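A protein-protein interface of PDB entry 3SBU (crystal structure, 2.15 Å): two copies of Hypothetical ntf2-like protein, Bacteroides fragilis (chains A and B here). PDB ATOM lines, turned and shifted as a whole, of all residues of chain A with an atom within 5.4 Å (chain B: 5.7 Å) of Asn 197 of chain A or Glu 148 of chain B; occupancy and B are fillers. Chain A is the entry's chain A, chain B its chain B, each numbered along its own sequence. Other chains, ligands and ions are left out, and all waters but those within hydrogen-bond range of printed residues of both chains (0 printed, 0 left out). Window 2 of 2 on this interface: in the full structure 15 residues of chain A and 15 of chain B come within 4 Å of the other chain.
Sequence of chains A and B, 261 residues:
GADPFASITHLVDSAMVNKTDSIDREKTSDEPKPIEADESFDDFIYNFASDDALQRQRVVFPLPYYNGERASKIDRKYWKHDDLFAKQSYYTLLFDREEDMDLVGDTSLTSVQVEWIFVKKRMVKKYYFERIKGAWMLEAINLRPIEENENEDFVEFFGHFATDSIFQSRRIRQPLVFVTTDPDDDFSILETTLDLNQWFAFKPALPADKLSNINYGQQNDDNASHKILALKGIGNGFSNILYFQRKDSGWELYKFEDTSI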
ATOM      1  N   ASP A 195     -18.059 -14.835  22.045  1.00  0.00           N
ATOM      2  CA  ASP A 195     -18.730 -15.403  23.212  1.00  0.00           C
ATOM      3  C   ASP A 195     -19.394 -16.700  22.725  1.00  0.00           C
ATOM      4  O   ASP A 195     -19.283 -17.009  21.532  1.00  0.00           O
ATOM      5  CB  ASP A 195     -19.707 -14.423  23.898  1.00  0.00           C
ATOM      6  CG  ASP A 195     -20.900 -13.930  23.080  1.00  0.00           C
ATOM      7  OD1 ASP A 195     -21.278 -14.612  22.102  1.00  0.00           O
ATOM      8  OD2 ASP A 195     -21.491 -12.897  23.459  1.00  0.00           O
ATOM      9  N   LEU A 196     -20.051 -17.461  23.625  1.00  0.00           N
ATOM     10  CA  LEU A 196     -20.644 -18.745  23.254  1.00  0.00           C
ATOM     11  C   LEU A 196     -21.757 -18.599  22.202  1.00  0.00           C
ATOM     12  O   LEU A 196     -21.810 -19.420  21.286  1.00  0.00           O
ATOM     13  CB  LEU A 196     -21.141 -19.539  24.477  1.00  0.00           C
ATOM     14  CG  LEU A 196     -20.063 -20.023  25.476  1.00  0.00           C
ATOM     15  CD1 LEU A 196     -20.691 -20.778  26.630  1.00  0.00           C
ATOM     16  CD2 LEU A 196     -19.013 -20.914  24.813  1.00  0.00           C
ATOM     17  N   ASN A 197     -22.593 -17.558  22.290  1.00  0.00           N
ATOM     18  CA  ASN A 197     -23.652 -17.320  21.301  1.00  0.00           C
ATOM     19  C   ASN A 197     -23.063 -16.974  19.926  1.00  0.00           C
ATOM     20  O   ASN A 197     -23.600 -17.415  18.912  1.00  0.00           O
ATOM     21  CB  ASN A 197     -24.604 -16.211  21.766  1.00  0.00           C
ATOM     22  CG  ASN A 197     -25.463 -16.609  22.950  1.00  0.00           C
ATOM     23  OD1 ASN A 197     -25.837 -17.777  23.140  1.00  0.00           O
ATOM     24  ND2 ASN A 197     -25.797 -15.633  23.775  1.00  0.00           N
ATOM     25  N   GLN A 198     -21.940 -16.223  19.896  1.00  0.00           N
ATOM     26  CA  GLN A 198     -21.289 -15.856  18.653  1.00  0.00           C
ATOM     27  C   GLN A 198     -20.613 -17.080  18.035  1.00  0.00           C
ATOM     28  O   GLN A 198     -20.616 -17.219  16.815  1.00  0.00           O
ATOM     29  CB  GLN A 198     -20.286 -14.721  18.858  1.00  0.00           C
ATOM     30  CG  GLN A 198     -20.930 -13.378  19.197  1.00  0.00           C
ATOM     31  CD  GLN A 198     -19.871 -12.381  19.614  1.00  0.00           C
ATOM     32  OE1 GLN A 198     -19.045 -12.625  20.502  1.00  0.00           O
ATOM     33  NE2 GLN A 198     -19.771 -11.297  18.898  1.00  0.00           N
ATOM     34  N   TRP A 199     -20.067 -17.980  18.857  1.00  0.00           N
ATOM     35  CA  TRP A 199     -19.448 -19.205  18.342  1.00  0.00           C
ATOM     36  C   TRP A 199     -20.520 -20.074  17.636  1.00  0.00           C
ATOM     37  O   TRP A 199     -20.260 -20.614  16.560  1.00  0.00           O
ATOM     38  CB  TRP A 199     -18.726 -19.995  19.440  1.00  0.00           C
ATOM     39  CG  TRP A 199     -18.611 -21.466  19.137  1.00  0.00           C
ATOM     40  CD1 TRP A 199     -19.414 -22.463  19.601  1.00  0.00           C
ATOM     41  CD2 TRP A 199     -17.700 -22.083  18.210  1.00  0.00           C
ATOM     42  NE1 TRP A 199     -19.035 -23.669  19.057  1.00  0.00           N
ATOM     43  CE2 TRP A 199     -17.983 -23.467  18.203  1.00  0.00           C
ATOM     44  CE3 TRP A 199     -16.702 -21.592  17.346  1.00  0.00           C
ATOM     45  CZ2 TRP A 199     -17.270 -24.378  17.404  1.00  0.00           C
ATOM     46  CZ3 TRP A 199     -15.996 -22.492  16.559  1.00  0.00           C
ATOM     47  CH2 TRP A 199     -16.274 -23.866  16.594  1.00  0.00           C
ATOM     48  N   PHE A 200     -21.718 -20.176  18.217  1.00  0.00           N
ATOM     49  CA  PHE A 200     -22.778 -20.972  17.603  1.00  0.00           C
ATOM     50  C   PHE A 200     -23.204 -20.410  16.242  1.00  0.00           C
ATOM     51  O   PHE A 200     -23.494 -21.193  15.344  1.00  0.00           O
ATOM     52  CB  PHE A 200     -23.988 -21.147  18.547  1.00  0.00           C
ATOM     53  CG  PHE A 200     -23.686 -22.077  19.705  1.00  0.00           C
ATOM     54  CD1 PHE A 200     -22.948 -23.248  19.510  1.00  0.00           C
ATOM     55  CD2 PHE A 200     -24.163 -21.802  20.981  1.00  0.00           C
ATOM     56  CE1 PHE A 200     -22.650 -24.093  20.575  1.00  0.00           C
ATOM     57  CE2 PHE A 200     -23.895 -22.669  22.041  1.00  0.00           C
ATOM     58  CZ  PHE A 200     -23.121 -23.799  21.830  1.00  0.00           C
ATOM     59  N   ALA A 201     -23.115 -19.083  16.053  1.00  0.00           N
ATOM     60  CA  ALA A 201     -23.470 -18.418  14.809  1.00  0.00           C
ATOM     61  C   ALA A 201     -22.356 -18.481  13.741  1.00  0.00           C
ATOM     62  O   ALA A 201     -22.660 -18.473  12.549  1.00  0.00           O
ATOM     63  CB  ALA A 201     -23.823 -16.963  15.095  1.00  0.00           C
ATOM     64  N   ILE B 146     -20.504  -9.600  14.741  1.00  0.00           N
ATOM     65  CA  ILE B 146     -21.870  -9.269  15.136  1.00  0.00           C
ATOM     66  C   ILE B 146     -22.222 -10.064  16.436  1.00  0.00           C
ATOM     67  O   ILE B 146     -21.799 -11.210  16.597  1.00  0.00           O
ATOM     68  CB  ILE B 146     -22.825  -9.565  13.946  1.00  0.00           C
ATOM     69  CG1 ILE B 146     -24.197  -8.870  14.109  1.00  0.00           C
ATOM     70  CG2 ILE B 146     -22.924 -11.070  13.599  1.00  0.00           C
ATOM     71  CD1 ILE B 146     -24.829  -8.605  12.831  1.00  0.00           C
ATOM     72  N   GLU B 147     -22.906  -9.404  17.372  1.00  0.00           N
ATOM     73  CA  GLU B 147     -23.354  -9.922  18.678  1.00  0.00           C
ATOM     74  C   GLU B 147     -24.825 -10.264  18.670  1.00  0.00           C
ATOM     75  O   GLU B 147     -25.506 -10.138  17.647  1.00  0.00           O
ATOM     76  CB  GLU B 147     -23.205  -8.820  19.751  1.00  0.00           C
ATOM     77  CG  GLU B 147     -21.823  -8.526  20.299  1.00  0.00           C
ATOM     78  CD  GLU B 147     -21.830  -7.308  21.214  1.00  0.00           C
ATOM     79  OE1 GLU B 147     -22.909  -6.690  21.393  1.00  0.00           O
ATOM     80  OE2 GLU B 147     -20.742  -6.949  21.725  1.00  0.00           O
ATOM     81  N   GLU B 148     -25.320 -10.629  19.852  1.00  0.00           N
ATOM     82  CA  GLU B 148     -26.728 -10.913  20.116  1.00  0.00           C
ATOM     83  C   GLU B 148     -27.502  -9.583  20.098  1.00  0.00           C
ATOM     84  O   GLU B 148     -26.928  -8.547  20.463  1.00  0.00           O
ATOM     85  CB  GLU B 148     -26.911 -11.670  21.460  1.00  0.00           C
ATOM     86  CG  GLU B 148     -25.926 -11.331  22.577  1.00  0.00           C
ATOM     87  CD  GLU B 148     -24.593 -12.063  22.568  1.00  0.00           C
ATOM     88  OE1 GLU B 148     -23.652 -11.556  21.919  1.00  0.00           O
ATOM     89  OE2 GLU B 148     -24.471 -13.111  23.246  1.00  0.00           O
ATOM     90  N   ASN B 149     -28.774  -9.597  19.645  1.00  0.00           N
ATOM     91  CA  ASN B 149     -29.660  -8.424  19.571  1.00  0.00           C
ATOM     92  C   ASN B 149     -29.075  -7.337  18.648  1.00  0.00           C
ATOM     93  O   ASN B 149     -29.097  -6.136  18.952  1.00  0.00           O
ATOM     94  CB  ASN B 149     -29.980  -7.892  20.971  1.00  0.00           C
ATOM     95  CG  ASN B 149     -30.587  -8.964  21.824  1.00  0.00           C
ATOM     96  OD1 ASN B 149     -31.335  -9.825  21.350  1.00  0.00           O
ATOM     97  ND2 ASN B 149     -30.169  -9.013  23.070  1.00  0.00           N
ATOM     98  N   GLU B 150     -28.568  -7.787  17.494  1.00  0.00           N
ATOM     99  CA  GLU B 150     -27.979  -6.930  16.478  1.00  0.00           C
ATOM    100  C   GLU B 150     -28.469  -7.325  15.095  1.00  0.00           C
ATOM    101  O   GLU B 150     -27.787  -7.066  14.101  1.00  0.00           O
ATOM    102  CB  GLU B 150     -26.451  -6.972  16.554  1.00  0.00           C
ATOM    103  CG  GLU B 150     -25.855  -6.104  17.639  1.00  0.00           C
ATOM    104  CD  GLU B 150     -24.400  -5.765  17.379  1.00  0.00           C
ATOM    105  OE1 GLU B 150     -23.649  -6.653  16.912  1.00  0.00           O
ATOM    106  OE2 GLU B 150     -24.009  -4.608  17.650  1.00  0.00           O
ATOM    107  N   GLU B 152     -28.732 -10.081  13.501  1.00  0.00           N
ATOM    108  CA  GLU B 152     -27.858 -10.979  12.753  1.00  0.00           C
ATOM    109  C   GLU B 152     -28.612 -11.847  11.732  1.00  0.00           C
ATOM    110  O   GLU B 152     -28.210 -11.852  10.574  1.00  0.00           O
ATOM    111  CB  GLU B 152     -27.036 -11.867  13.716  1.00  0.00           C
ATOM    112  CG  GLU B 152     -26.226 -12.939  13.014  1.00  0.00           C
ATOM    113  CD  GLU B 152     -25.295 -13.742  13.898  1.00  0.00           C
ATOM    114  OE1 GLU B 152     -25.606 -13.921  15.099  1.00  0.00           O
ATOM    115  OE2 GLU B 152     -24.243 -14.185  13.382  1.00  0.00           O
ATOM    116  N   ASN B 220     -34.219  -4.502  19.453  1.00  0.00           N
ATOM    117  CA  ASN B 220     -33.665  -5.177  18.252  1.00  0.00           C
ATOM    118  C   ASN B 220     -33.373  -6.625  18.685  1.00  0.00           C
ATOM    119  O   ASN B 220     -32.243  -7.095  18.601  1.00  0.00           O
ATOM    120  CB  ASN B 220     -32.403  -4.438  17.757  1.00  0.00           C
ATOM    121  CG  ASN B 220     -32.575  -3.317  16.730  1.00  0.00           C
ATOM    122  OD1 ASN B 220     -31.581  -2.889  16.161  1.00  0.00           O
ATOM    123  ND2 ASN B 220     -33.794  -2.789  16.453  1.00  0.00           N
ATOM    124  N   ASP B 222     -33.353 -10.712  18.950  1.00  0.00           N
ATOM    125  CA  ASP B 222     -33.111 -11.826  18.033  1.00  0.00           C
ATOM    126  C   ASP B 222     -34.361 -12.679  17.809  1.00  0.00           C
ATOM    127  O   ASP B 222     -34.493 -13.257  16.731  1.00  0.00           O
ATOM    128  CB  ASP B 222     -31.943 -12.706  18.509  1.00  0.00           C
ATOM    129  CG  ASP B 222     -30.592 -12.030  18.359  1.00  0.00           C
ATOM    130  OD1 ASP B 222     -30.351 -11.373  17.287  1.00  0.00           O
ATOM    131  OD2 ASP B 222     -29.751 -12.199  19.259  1.00  0.00           O
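Among the printed residues, merely in contact across the chains: Gln 198 of chain A with Glu 147 of chain B and Ala 201 of chain A with Glu 152 of chain B.
Printed residues of chain B within 4 Å of Asp 195 of chain A: Glu 148.
Of the printed residues of chain B, Ala 201 of chain A touches Glu 152.
Printed residues of chain A within 4 Å of Glu 148 of chain B: Asp 195 (3.0 Å) and Asn 197 (2.9 Å).
Glu 150 of chain B touches none of the printed residues of chain A.
Of the printed residues of chain A, Glu 152 of chain B touches Ala 201 (3.3 Å).
The side-chain carboxylate of Glu 148 of chain B lies within hydrogen-bond range of the side-chain amide nitrogen of Asn 197 of chain A.
The side-chain amide nitrogen (NE2) of Gln 198 of chain A is in hydrogen-bond range of the backbone carbonyl oxygen (O) of Ile 146 of chain B, at 3.1 Å.
The side-chain carboxylate (OD2) of Asp 195 of chain A sits close to the side-chain carboxylate (OE1) of Glu 148 of chain B (3.0 Å).
No position is printed for both chains.
Of the 5 pairs that touch across the chains among the printed residues, none has its exchanged pair printed and touching as well.
OD1 of Asp 195 of chain A lies within hydrogen-bond range of N of Asn 197 of chain A, 3.2 Å away.
The backbone NH (N) of Gln 198 of chain A lies within hydrogen-bond range of the side-chain carboxylate (OD1) of Asp 195 of chain A (2.8 Å).
The backbone NH (N) of Glu 147 of chain B sits at hydrogen-bond distance from the side-chain carboxylate (OE1) of Glu 150 of chain B.
Of the 7 printed residues of chain A, 4 touch a printed residue of chain B.
Printed residues of chain A that touch a printed residue of chain B: Asp 195, Asn 197, Gln 198 and Ala 201.
Hydrophobic or aromatic side chains of chain A that line the printed part of chain B: Ala 201.
Printed residues of chain B that touch a printed residue of chain A: Ile 146, Glu 147, Glu 148 and Glu 152.
Among the printed residues, no Asp or Glu carboxylate lies within 4 Å of a Lys or Arg side-chain nitrogen of the other chain.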
